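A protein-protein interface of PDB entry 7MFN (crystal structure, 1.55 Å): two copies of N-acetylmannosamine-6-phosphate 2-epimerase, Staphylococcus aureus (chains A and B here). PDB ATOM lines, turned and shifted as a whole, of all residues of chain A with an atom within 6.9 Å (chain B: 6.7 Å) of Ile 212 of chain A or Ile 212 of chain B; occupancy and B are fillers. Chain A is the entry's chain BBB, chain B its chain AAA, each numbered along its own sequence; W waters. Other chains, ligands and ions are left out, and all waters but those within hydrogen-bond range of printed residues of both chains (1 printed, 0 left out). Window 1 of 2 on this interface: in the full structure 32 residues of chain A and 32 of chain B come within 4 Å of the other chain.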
ATOM      1  N   LEU A   6     -17.644  26.232  36.693  1.00  0.00           N
ATOM      2  CA  LEU A   6     -17.127  25.212  35.748  1.00  0.00           C
ATOM      3  C   LEU A   6     -15.607  25.301  35.593  1.00  0.00           C
ATOM      4  O   LEU A   6     -15.077  26.358  35.173  1.00  0.00           O
ATOM      5  CB  LEU A   6     -17.801  25.371  34.390  1.00  0.00           C
ATOM      6  CG  LEU A   6     -17.396  24.357  33.308  1.00  0.00           C
ATOM      7  CD1 LEU A   6     -17.941  22.996  33.663  1.00  0.00           C
ATOM      8  CD2 LEU A   6     -17.906  24.843  31.967  1.00  0.00           C
ATOM      9  N   GLY A  34     -15.899  31.102  26.938  1.00  0.00           N
ATOM     10  CA  GLY A  34     -17.219  30.518  27.175  1.00  0.00           C
ATOM     11  C   GLY A  34     -17.746  30.615  28.604  1.00  0.00           C
ATOM     12  O   GLY A  34     -18.899  30.221  28.793  1.00  0.00           O
ATOM     13  N   PRO A 186     -24.379  18.936  30.065  1.00  0.00           N
ATOM     14  CA  PRO A 186     -24.855  20.038  30.901  1.00  0.00           C
ATOM     15  C   PRO A 186     -25.835  19.567  31.979  1.00  0.00           C
ATOM     16  O   PRO A 186     -25.790  20.040  33.112  1.00  0.00           O
ATOM     17  CB  PRO A 186     -25.473  20.974  29.860  1.00  0.00           C
ATOM     18  CG  PRO A 186     -24.614  20.768  28.604  1.00  0.00           C
ATOM     19  CD  PRO A 186     -24.407  19.264  28.614  1.00  0.00           C
ATOM     20  N   VAL A 202     -15.098  19.439  33.892  1.00  0.00           N
ATOM     21  CA  VAL A 202     -15.541  18.809  32.630  1.00  0.00           C
ATOM     22  C   VAL A 202     -14.354  18.884  31.677  1.00  0.00           C
ATOM     23  O   VAL A 202     -13.825  19.977  31.422  1.00  0.00           O
ATOM     24  CB  VAL A 202     -16.746  19.551  32.032  1.00  0.00           C
ATOM     25  CG1 VAL A 202     -17.106  18.963  30.656  1.00  0.00           C
ATOM     26  CG2 VAL A 202     -17.953  19.466  32.980  1.00  0.00           C
ATOM     27  N   GLY A 203     -13.920  17.721  31.206  1.00  0.00           N
ATOM     28  CA  GLY A 203     -12.768  17.628  30.306  1.00  0.00           C
ATOM     29  C   GLY A 203     -13.186  17.170  28.927  1.00  0.00           C
ATOM     30  O   GLY A 203     -13.449  18.026  28.055  1.00  0.00           O
ATOM     31  N   GLY A 204     -13.278  15.867  28.715  1.00  0.00           N
ATOM     32  CA  GLY A 204     -13.436  15.310  27.364  1.00  0.00           C
ATOM     33  C   GLY A 204     -14.694  15.793  26.665  1.00  0.00           C
ATOM     34  O   GLY A 204     -14.646  15.887  25.420  1.00  0.00           O
ATOM     35  N   ALA A 205     -15.766  16.091  27.364  1.00  0.00           N
ATOM     36  CA  ALA A 205     -17.003  16.574  26.745  1.00  0.00           C
ATOM     37  C   ALA A 205     -16.806  17.952  26.111  1.00  0.00           C
ATOM     38  O   ALA A 205     -17.673  18.353  25.304  1.00  0.00           O
ATOM     39  CB  ALA A 205     -18.111  16.601  27.758  1.00  0.00           C
ATOM     40  N   ILE A 206     -15.770  18.688  26.446  1.00  0.00           N
ATOM     41  CA  ILE A 206     -15.476  19.996  25.840  1.00  0.00           C
ATOM     42  C   ILE A 206     -14.221  19.932  24.977  1.00  0.00           C
ATOM     43  O   ILE A 206     -14.207  20.535  23.898  1.00  0.00           O
ATOM     44  CB  ILE A 206     -15.377  21.072  26.948  1.00  0.00           C
ATOM     45  CG1 ILE A 206     -16.735  21.253  27.645  1.00  0.00           C
ATOM     46  CG2 ILE A 206     -14.892  22.385  26.349  1.00  0.00           C
ATOM     47  CD1 ILE A 206     -16.692  22.095  28.925  1.00  0.00           C
ATOM     48  N   THR A 207     -13.153  19.250  25.428  1.00  0.00           N
ATOM     49  CA  THR A 207     -11.794  19.362  24.868  1.00  0.00           C
ATOM     50  C   THR A 207     -11.254  18.067  24.237  1.00  0.00           C
ATOM     51  O   THR A 207     -10.154  18.137  23.733  1.00  0.00           O
ATOM     52  CB  THR A 207     -10.809  19.885  25.908  1.00  0.00           C
ATOM     53  OG1 THR A 207     -10.666  18.913  26.943  1.00  0.00           O
ATOM     54  CG2 THR A 207     -11.242  21.230  26.458  1.00  0.00           C
ATOM     55  N   ARG A 208     -12.071  17.026  24.093  1.00  0.00           N
ATOM     56  CA  ARG A 208     -11.650  15.802  23.361  1.00  0.00           C
ATOM     57  C   ARG A 208     -12.618  15.534  22.209  1.00  0.00           C
ATOM     58  O   ARG A 208     -13.550  14.733  22.336  1.00  0.00           O
ATOM     59  CB  ARG A 208     -11.565  14.608  24.292  1.00  0.00           C
ATOM     60  CG  ARG A 208     -10.344  14.624  25.195  1.00  0.00           C
ATOM     61  CD  ARG A 208     -10.163  13.324  25.985  1.00  0.00           C
ATOM     62  NE  ARG A 208      -8.855  13.321  26.621  1.00  0.00           N
ATOM     63  CZ  ARG A 208      -8.608  13.382  27.936  1.00  0.00           C
ATOM     64  NH1 ARG A 208      -9.585  13.390  28.828  1.00  0.00           N
ATOM     65  NH2 ARG A 208      -7.343  13.436  28.307  1.00  0.00           N
ATOM     66  N   PRO A 209     -12.423  16.192  21.058  1.00  0.00           N
ATOM     67  CA  PRO A 209     -13.295  15.935  19.919  1.00  0.00           C
ATOM     68  C   PRO A 209     -13.422  14.452  19.562  1.00  0.00           C
ATOM     69  O   PRO A 209     -14.493  14.062  19.071  1.00  0.00           O
ATOM     70  CB  PRO A 209     -12.669  16.752  18.795  1.00  0.00           C
ATOM     71  CG  PRO A 209     -11.262  17.015  19.256  1.00  0.00           C
ATOM     72  CD  PRO A 209     -11.423  17.207  20.753  1.00  0.00           C
ATOM     73  N   LYS A 210     -12.387  13.642  19.755  1.00  0.00           N
ATOM     74  CA  LYS A 210     -12.535  12.184  19.444  1.00  0.00           C
ATOM     75  C   LYS A 210     -13.640  11.565  20.315  1.00  0.00           C
ATOM     76  O   LYS A 210     -14.456  10.799  19.845  1.00  0.00           O
ATOM     77  CB  LYS A 210     -11.231  11.449  19.656  1.00  0.00           C
ATOM     78  CG  LYS A 210     -11.302   9.954  19.438  1.00  0.00           C
ATOM     79  CD  LYS A 210      -9.925   9.377  19.667  1.00  0.00           C
ATOM     80  CE  LYS A 210      -9.968   7.879  19.676  1.00  0.00           C
ATOM     81  NZ  LYS A 210      -8.578   7.390  19.786  1.00  0.00           N
ATOM     82  N   GLU A 211     -13.678  11.917  21.608  1.00  0.00           N
ATOM     83  CA  GLU A 211     -14.660  11.328  22.533  1.00  0.00           C
ATOM     84  C   GLU A 211     -16.048  11.887  22.245  1.00  0.00           C
ATOM     85  O   GLU A 211     -17.019  11.159  22.365  1.00  0.00           O
ATOM     86  CB  GLU A 211     -14.202  11.589  23.956  1.00  0.00           C
ATOM     87  CG  GLU A 211     -12.918  10.858  24.260  1.00  0.00           C
ATOM     88  CD  GLU A 211     -13.057   9.345  24.109  1.00  0.00           C
ATOM     89  OE1 GLU A 211     -14.056   8.769  24.615  1.00  0.00           O
ATOM     90  OE2 GLU A 211     -12.204   8.745  23.451  1.00  0.00           O
ATOM     91  N   ILE A 212     -16.142  13.157  21.867  1.00  0.00           N
ATOM     92  CA  ILE A 212     -17.472  13.716  21.520  1.00  0.00           C
ATOM     93  C   ILE A 212     -17.981  13.045  20.238  1.00  0.00           C
ATOM     94  O   ILE A 212     -19.132  12.618  20.189  1.00  0.00           O
ATOM     95  CB  ILE A 212     -17.446  15.251  21.384  1.00  0.00           C
ATOM     96  CG1 ILE A 212     -16.835  15.944  22.591  1.00  0.00           C
ATOM     97  CG2 ILE A 212     -18.828  15.768  21.109  1.00  0.00           C
ATOM     98  CD1 ILE A 212     -16.469  17.370  22.349  1.00  0.00           C
ATOM     99  N   THR A 213     -17.084  12.876  19.262  1.00  0.00           N
ATOM    100  CA  THR A 213     -17.445  12.214  17.981  1.00  0.00           C
ATOM    101  C   THR A 213     -17.968  10.819  18.319  1.00  0.00           C
ATOM    102  O   THR A 213     -18.998  10.413  17.780  1.00  0.00           O
ATOM    103  CB  THR A 213     -16.246  12.166  17.034  1.00  0.00           C
ATOM    104  OG1 THR A 213     -15.868  13.499  16.683  1.00  0.00           O
ATOM    105  CG2 THR A 213     -16.583  11.415  15.766  1.00  0.00           C
ATOM    106  N   LYS A 214     -17.219  10.084  19.136  1.00  0.00           N
ATOM    107  CA  LYS A 214     -17.596   8.695  19.496  1.00  0.00           C
ATOM    108  C   LYS A 214     -19.014   8.673  20.078  1.00  0.00           C
ATOM    109  O   LYS A 214     -19.757   7.690  19.829  1.00  0.00           O
ATOM    110  CB  LYS A 214     -16.594   8.084  20.471  1.00  0.00           C
ATOM    111  CG  LYS A 214     -15.275   7.669  19.859  1.00  0.00           C
ATOM    112  CD  LYS A 214     -14.212   7.306  20.893  1.00  0.00           C
ATOM    113  CE  LYS A 214     -14.660   6.287  21.910  1.00  0.00           C
ATOM    114  NZ  LYS A 214     -13.526   5.965  22.811  1.00  0.00           N
ATOM    115  N   ARG A 215     -19.408   9.710  20.830  1.00  0.00           N
ATOM    116  CA  ARG A 215     -20.756   9.752  21.443  1.00  0.00           C
ATOM    117  C   ARG A 215     -21.845   9.967  20.389  1.00  0.00           C
ATOM    118  O   ARG A 215     -22.901   9.394  20.554  1.00  0.00           O
ATOM    119  CB  ARG A 215     -20.775  10.800  22.556  1.00  0.00           C
ATOM    120  CG  ARG A 215     -20.625  10.190  23.940  1.00  0.00           C
ATOM    121  CD  ARG A 215     -21.027  11.171  25.031  1.00  0.00           C
ATOM    122  NE  ARG A 215     -20.193  12.367  24.975  1.00  0.00           N
ATOM    123  CZ  ARG A 215     -20.627  13.625  24.747  1.00  0.00           C
ATOM    124  NH1 ARG A 215     -19.752  14.599  24.676  1.00  0.00           N
ATOM    125  NH2 ARG A 215     -21.891  13.904  24.530  1.00  0.00           N
ATOM    126  N   PHE A 216     -21.591  10.790  19.369  1.00  0.00           N
ATOM    127  CA  PHE A 216     -22.491  10.987  18.227  1.00  0.00           C
ATOM    128  C   PHE A 216     -22.615   9.680  17.462  1.00  0.00           C
ATOM    129  O   PHE A 216     -23.714   9.252  17.121  1.00  0.00           O
ATOM    130  CB  PHE A 216     -22.029  12.128  17.314  1.00  0.00           C
ATOM    131  CG  PHE A 216     -22.451  13.490  17.833  1.00  0.00           C
ATOM    132  CD1 PHE A 216     -21.758  14.146  18.847  1.00  0.00           C
ATOM    133  CD2 PHE A 216     -23.538  14.111  17.275  1.00  0.00           C
ATOM    134  CE1 PHE A 216     -22.194  15.384  19.303  1.00  0.00           C
ATOM    135  CE2 PHE A 216     -23.970  15.357  17.732  1.00  0.00           C
ATOM    136  CZ  PHE A 216     -23.278  15.998  18.721  1.00  0.00           C
ATOM    137  N   VAL A 217     -21.491   9.062  17.134  1.00  0.00           N
ATOM    138  CA  VAL A 217     -21.569   7.807  16.333  1.00  0.00           C
ATOM    139  C   VAL A 217     -22.321   6.708  17.108  1.00  0.00           C
ATOM    140  O   VAL A 217     -23.141   6.010  16.510  1.00  0.00           O
ATOM    141  CB  VAL A 217     -20.141   7.386  15.965  1.00  0.00           C
ATOM    142  CG1 VAL A 217     -20.089   5.989  15.368  1.00  0.00           C
ATOM    143  CG2 VAL A 217     -19.446   8.380  15.056  1.00  0.00           C
ATOM    144  N   LEU B   6     -21.743  10.452   9.858  1.00  0.00           N
ATOM    145  CA  LEU B   6     -21.413  11.747  10.487  1.00  0.00           C
ATOM    146  C   LEU B   6     -20.296  12.435   9.728  1.00  0.00           C
ATOM    147  O   LEU B   6     -19.160  11.842   9.645  1.00  0.00           O
ATOM    148  CB  LEU B   6     -21.033  11.485  11.933  1.00  0.00           C
ATOM    149  CG  LEU B   6     -20.648  12.723  12.762  1.00  0.00           C
ATOM    150  CD1 LEU B   6     -21.881  13.559  13.015  1.00  0.00           C
ATOM    151  CD2 LEU B   6     -20.012  12.298  14.075  1.00  0.00           C
ATOM    152  N   PRO B 186     -26.159  14.300  20.235  1.00  0.00           N
ATOM    153  CA  PRO B 186     -26.395  12.993  19.651  1.00  0.00           C
ATOM    154  C   PRO B 186     -27.870  12.688  19.374  1.00  0.00           C
ATOM    155  O   PRO B 186     -28.232  12.138  18.359  1.00  0.00           O
ATOM    156  CB  PRO B 186     -25.814  12.061  20.706  1.00  0.00           C
ATOM    157  CG  PRO B 186     -24.669  12.830  21.215  1.00  0.00           C
ATOM    158  CD  PRO B 186     -25.202  14.245  21.373  1.00  0.00           C
ATOM    159  N   VAL B 202     -21.981  17.915  11.781  1.00  0.00           N
ATOM    160  CA  VAL B 202     -21.879  18.433  13.167  1.00  0.00           C
ATOM    161  C   VAL B 202     -20.558  19.198  13.243  1.00  0.00           C
ATOM    162  O   VAL B 202     -19.497  18.633  12.919  1.00  0.00           O
ATOM    163  CB  VAL B 202     -21.998  17.308  14.195  1.00  0.00           C
ATOM    164  CG1 VAL B 202     -21.708  17.864  15.589  1.00  0.00           C
ATOM    165  CG2 VAL B 202     -23.354  16.615  14.138  1.00  0.00           C
ATOM    166  N   GLY B 203     -20.622  20.472  13.669  1.00  0.00           N
ATOM    167  CA  GLY B 203     -19.453  21.324  13.762  1.00  0.00           C
ATOM    168  C   GLY B 203     -19.147  21.715  15.193  1.00  0.00           C
ATOM    169  O   GLY B 203     -18.412  20.975  15.901  1.00  0.00           O
ATOM    170  N   GLY B 204     -19.768  22.810  15.603  1.00  0.00           N
ATOM    171  CA  GLY B 204     -19.456  23.427  16.918  1.00  0.00           C
ATOM    172  C   GLY B 204     -19.602  22.475  18.087  1.00  0.00           C
ATOM    173  O   GLY B 204     -18.787  22.610  19.063  1.00  0.00           O
ATOM    174  N   ALA B 205     -20.528  21.529  18.062  1.00  0.00           N
ATOM    175  CA  ALA B 205     -20.757  20.625  19.202  1.00  0.00           C
ATOM    176  C   ALA B 205     -19.578  19.657  19.339  1.00  0.00           C
ATOM    177  O   ALA B 205     -19.494  19.008  20.386  1.00  0.00           O
ATOM    178  CB  ALA B 205     -22.044  19.896  19.036  1.00  0.00           C
ATOM    179  N   ILE B 206     -18.689  19.556  18.364  1.00  0.00           N
ATOM    180  CA  ILE B 206     -17.462  18.713  18.463  1.00  0.00           C
ATOM    181  C   ILE B 206     -16.211  19.560  18.439  1.00  0.00           C
ATOM    182  O   ILE B 206     -15.286  19.226  19.203  1.00  0.00           O
ATOM    183  CB  ILE B 206     -17.484  17.658  17.324  1.00  0.00           C
ATOM    184  CG1 ILE B 206     -18.695  16.741  17.476  1.00  0.00           C
ATOM    185  CG2 ILE B 206     -16.173  16.883  17.298  1.00  0.00           C
ATOM    186  CD1 ILE B 206     -18.905  15.779  16.345  1.00  0.00           C
ATOM    187  N   THR B 207     -16.144  20.612  17.609  1.00  0.00           N
ATOM    188  CA  THR B 207     -14.873  21.303  17.315  1.00  0.00           C
ATOM    189  C   THR B 207     -14.845  22.776  17.748  1.00  0.00           C
ATOM    190  O   THR B 207     -13.837  23.397  17.431  1.00  0.00           O
ATOM    191  CB  THR B 207     -14.551  21.206  15.815  1.00  0.00           C
ATOM    192  OG1 THR B 207     -15.559  21.858  15.052  1.00  0.00           O
ATOM    193  CG2 THR B 207     -14.437  19.764  15.363  1.00  0.00           C
ATOM    194  N   ARG B 208     -15.852  23.268  18.478  1.00  0.00           N
ATOM    195  CA  ARG B 208     -15.844  24.641  19.053  1.00  0.00           C
ATOM    196  C   ARG B 208     -15.978  24.577  20.567  1.00  0.00           C
ATOM    197  O   ARG B 208     -17.070  24.697  21.122  1.00  0.00           O
ATOM    198  CB  ARG B 208     -16.884  25.554  18.428  1.00  0.00           C
ATOM    199  CG  ARG B 208     -16.480  26.011  17.037  1.00  0.00           C
ATOM    200  CD  ARG B 208     -17.468  27.018  16.468  1.00  0.00           C
ATOM    201  NE  ARG B 208     -16.923  27.604  15.263  1.00  0.00           N
ATOM    202  CZ  ARG B 208     -17.424  27.464  14.041  1.00  0.00           C
ATOM    203  NH1 ARG B 208     -16.760  27.999  13.032  1.00  0.00           N
ATOM    204  NH2 ARG B 208     -18.515  26.753  13.847  1.00  0.00           N
ATOM    205  N   PRO B 209     -14.865  24.312  21.280  1.00  0.00           N
ATOM    206  CA  PRO B 209     -14.930  24.230  22.746  1.00  0.00           C
ATOM    207  C   PRO B 209     -15.557  25.469  23.399  1.00  0.00           C
ATOM    208  O   PRO B 209     -16.190  25.315  24.453  1.00  0.00           O
ATOM    209  CB  PRO B 209     -13.476  24.013  23.172  1.00  0.00           C
ATOM    210  CG  PRO B 209     -12.664  24.483  22.000  1.00  0.00           C
ATOM    211  CD  PRO B 209     -13.499  24.062  20.797  1.00  0.00           C
ATOM    212  N   LYS B 210     -15.407  26.652  22.811  1.00  0.00           N
ATOM    213  CA  LYS B 210     -16.077  27.834  23.416  1.00  0.00           C
ATOM    214  C   LYS B 210     -17.584  27.642  23.415  1.00  0.00           C
ATOM    215  O   LYS B 210     -18.272  27.970  24.386  1.00  0.00           O
ATOM    216  CB  LYS B 210     -15.706  29.101  22.636  1.00  0.00           C
ATOM    217  CG  LYS B 210     -16.363  30.357  23.166  1.00  0.00           C
ATOM    218  CD  LYS B 210     -15.972  31.526  22.267  1.00  0.00           C
ATOM    219  CE  LYS B 210     -16.742  32.761  22.647  1.00  0.00           C
ATOM    220  NZ  LYS B 210     -16.230  33.904  21.862  1.00  0.00           N
ATOM    221  N   GLU B 211     -18.117  27.170  22.287  1.00  0.00           N
ATOM    222  CA  GLU B 211     -19.561  26.943  22.108  1.00  0.00           C
ATOM    223  C   GLU B 211     -20.038  25.880  23.106  1.00  0.00           C
ATOM    224  O   GLU B 211     -21.057  26.070  23.748  1.00  0.00           O
ATOM    225  CB  GLU B 211     -19.834  26.530  20.653  1.00  0.00           C
ATOM    226  CG  GLU B 211     -21.274  26.238  20.352  1.00  0.00           C
ATOM    227  CD  GLU B 211     -21.514  25.802  18.918  1.00  0.00           C
ATOM    228  OE1 GLU B 211     -21.058  26.528  18.015  1.00  0.00           O
ATOM    229  OE2 GLU B 211     -22.092  24.723  18.718  1.00  0.00           O
ATOM    230  N   ILE B 212     -19.293  24.770  23.259  1.00  0.00           N
ATOM    231  CA  ILE B 212     -19.687  23.672  24.172  1.00  0.00           C
ATOM    232  C   ILE B 212     -19.650  24.206  25.614  1.00  0.00           C
ATOM    233  O   ILE B 212     -20.595  23.968  26.381  1.00  0.00           O
ATOM    234  CB  ILE B 212     -18.791  22.424  23.977  1.00  0.00           C
ATOM    235  CG1 ILE B 212     -18.741  21.968  22.517  1.00  0.00           C
ATOM    236  CG2 ILE B 212     -19.277  21.316  24.857  1.00  0.00           C
ATOM    237  CD1 ILE B 212     -17.595  20.998  22.215  1.00  0.00           C
ATOM    238  N   THR B 213     -18.600  24.934  25.932  1.00  0.00           N
ATOM    239  CA  THR B 213     -18.461  25.498  27.290  1.00  0.00           C
ATOM    240  C   THR B 213     -19.683  26.368  27.588  1.00  0.00           C
ATOM    241  O   THR B 213     -20.272  26.263  28.675  1.00  0.00           O
ATOM    242  CB  THR B 213     -17.207  26.318  27.400  1.00  0.00           C
ATOM    243  OG1 THR B 213     -16.046  25.503  27.228  1.00  0.00           O
ATOM    244  CG2 THR B 213     -17.044  26.977  28.750  1.00  0.00           C
ATOM    245  N   LYS B 214     -20.071  27.233  26.646  1.00  0.00           N
ATOM    246  CA  LYS B 214     -21.261  28.107  26.841  1.00  0.00           C
ATOM    247  C   LYS B 214     -22.504  27.263  27.179  1.00  0.00           C
ATOM    248  O   LYS B 214     -23.314  27.661  28.066  1.00  0.00           O
ATOM    249  CB  LYS B 214     -21.568  28.954  25.606  1.00  0.00           C
ATOM    250  CG  LYS B 214     -20.680  30.167  25.406  1.00  0.00           C
ATOM    251  CD  LYS B 214     -21.076  31.044  24.206  1.00  0.00           C
ATOM    252  CE  LYS B 214     -20.779  32.510  24.464  1.00  0.00           C
ATOM    253  NZ  LYS B 214     -20.616  33.305  23.227  1.00  0.00           N
ATOM    254  N   ARG B 215     -22.697  26.098  26.548  1.00  0.00           N
ATOM    255  CA  ARG B 215     -23.880  25.254  26.857  1.00  0.00           C
ATOM    256  C   ARG B 215     -23.820  24.734  28.290  1.00  0.00           C
ATOM    257  O   ARG B 215     -24.862  24.696  28.962  1.00  0.00           O
ATOM    258  CB  ARG B 215     -24.009  24.048  25.926  1.00  0.00           C
ATOM    259  CG  ARG B 215     -24.748  24.330  24.629  1.00  0.00           C
ATOM    260  CD  ARG B 215     -25.062  23.035  23.877  1.00  0.00           C
ATOM    261  NE  ARG B 215     -25.940  22.081  24.587  1.00  0.00           N
ATOM    262  CZ  ARG B 215     -25.733  20.769  24.803  1.00  0.00           C
ATOM    263  NH1 ARG B 215     -26.623  20.041  25.463  1.00  0.00           N
ATOM    264  NH2 ARG B 215     -24.638  20.183  24.385  1.00  0.00           N
ATOM    265  N   PHE B 216     -22.636  24.368  28.761  1.00  0.00           N
ATOM    266  CA  PHE B 216     -22.505  23.954  30.179  1.00  0.00           C
ATOM    267  C   PHE B 216     -22.828  25.124  31.106  1.00  0.00           C
ATOM    268  O   PHE B 216     -23.579  24.986  32.059  1.00  0.00           O
ATOM    269  CB  PHE B 216     -21.124  23.364  30.444  1.00  0.00           C
ATOM    270  CG  PHE B 216     -21.002  21.920  30.033  1.00  0.00           C
ATOM    271  CD1 PHE B 216     -20.729  21.559  28.725  1.00  0.00           C
ATOM    272  CD2 PHE B 216     -21.122  20.924  30.991  1.00  0.00           C
ATOM    273  CE1 PHE B 216     -20.633  20.229  28.352  1.00  0.00           C
ATOM    274  CE2 PHE B 216     -21.015  19.594  30.620  1.00  0.00           C
ATOM    275  CZ  PHE B 216     -20.736  19.266  29.315  1.00  0.00           C
ATOM    276  N   VAL B 217     -22.240  26.272  30.827  1.00  0.00           N
ATOM    277  CA  VAL B 217     -22.454  27.438  31.748  1.00  0.00           C
ATOM    278  C   VAL B 217     -23.946  27.817  31.737  1.00  0.00           C
ATOM    279  O   VAL B 217     -24.492  28.128  32.815  1.00  0.00           O
ATOM    280  CB  VAL B 217     -21.535  28.581  31.331  1.00  0.00           C
ATOM    281  CG1 VAL B 217     -21.904  29.895  32.055  1.00  0.00           C
ATOM    282  CG2 VAL B 217     -20.084  28.237  31.550  1.00  0.00           C
HETATM  283  O   HOH W   1     -13.366  20.299  21.109  1.00  0.00           O
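O of Pro 209 of chain A sits at hydrogen-bond distance from OG1 of Thr 213 of chain A. The backbone carbonyl oxygen (O) of Pro 209 of chain B lies within hydrogen-bond range of the side-chain hydroxyl (OG1) of Thr 213 of chain B, 2.8 Å away.
Among the printed residues, merely in contact across the chains: Ile 212 of chain A with Ala 205 of chain B, Ala 205 of chain A with Ile 212 of chain B, Ile 206 of chain A with Thr 213 of chain B, Thr 213 of chain A with Ile 206 of chain B, Pro 186 of chain A with Phe 216 of chain B, Phe 216 of chain A with Pro 186 of chain B, Gly 34 of chain A with Val 217 of chain B, Pro 209 of chain A with Ile 206 of chain B, Ile 206 of chain A with Pro 209 of chain B, Gly 34 of chain A with Thr 213 of chain B, Gly 34 of chain A with Lys 214 of chain B, Ile 212 of chain A with Ile 206 of chain B, Ile 206 of chain A with Ile 212 of chain B, Pro 186 of chain A with Arg 215 of chain B, Ile 212 of chain A with Ile 212 of chain B, Phe 216 of chain A with Leu 6 of chain B, Leu 6 of chain A with Phe 216 of chain B, Phe 216 of chain A with Val 202 of chain B, Val 202 of chain A with Phe 216 of chain B, Gly 34 of chain A with Lys 210 of chain B, Arg 215 of chain A with Pro 186 of chain B, Thr 213 of chain A with Leu 6 of chain B and Leu 6 of chain A with Thr 213 of chain B.
Printed residues of chain B within 4 Å of Gly 34 of chain A: Lys 210, Thr 213, Lys 214 and Val 217. Of the printed residues of chain B, Ala 205 of chain A touches Ile 212. Arg 208 of chain A touches none of the printed residues of chain B. Ile 212 of chain A touches three residues of chain B. Arg 208 of chain B touches none of the printed residues of chain A. Of the printed residues of chain A, Pro 209 of chain B touches Ile 206. Of the printed residues of chain A, Thr 213 of chain B touches Leu 6, Gly 34 and Ile 206. The nearest residue of chain A that does not touch Ile 212 of chain B is Pro 186 of chain A (5.6 Å). The nearest printed residue of chain A that does not touch Pro 209 of chain B is Thr 207 of chain A (4.9 Å).
Hydrophobic or aromatic side chains of chain B within 4 Å of the printed part of chain A: Leu 6, Pro 186, Val 202, Ile 206, Pro 209, Ile 212, Phe 216 and Val 217. Of the 19 printed residues of chain A, 11 touch a printed residue of chain B. Printed residues of chain A that touch a printed residue of chain B: Leu 6, Gly 34, Pro 186, Val 202, Ala 205, Ile 206, Pro 209, Ile 212, Thr 213, Arg 215 and Phe 216. Hydrophobic or aromatic side chains of chain A that line the printed part of chain B: Leu 6, Pro 186, Val 202, Ile 206, Pro 209, Ile 212 and Phe 216. Among the printed residues, no Asp or Glu carboxylate lies within 4 Å of a Lys or Arg side-chain nitrogen of the other chain.
Val 202 of chain A touches Phe 216 of chain B, and with the chains exchanged Phe 216 of chain A touches Val 202 of chain B. Ala 205 of chain A touches Ile 212 of chain B, and with the chains exchanged Ile 212 of chain A touches Ala 205 of chain B. Ile 206 of chain A touches Ile 212 of chain B, and with the chains exchanged Ile 212 of chain A touches Ile 206 of chain B. Ile 212 of chain A touches its own counterpart, Ile 212 of chain B. Positions printed for both chains: 6, 186, 202, 203, 204, 205, 206, 207, 208, 209, 210, 211, 212, 213, 214, 215, 216 and 217. Of the 23 pairs that touch across the chains among the printed residues, 19 have their exchanged pair printed and touching as well.
Water W1 lies within hydrogen-bond range of O of Ile 206 of chain B (2.9 Å) and O of Ile 206 of chain A (2.9 Å).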
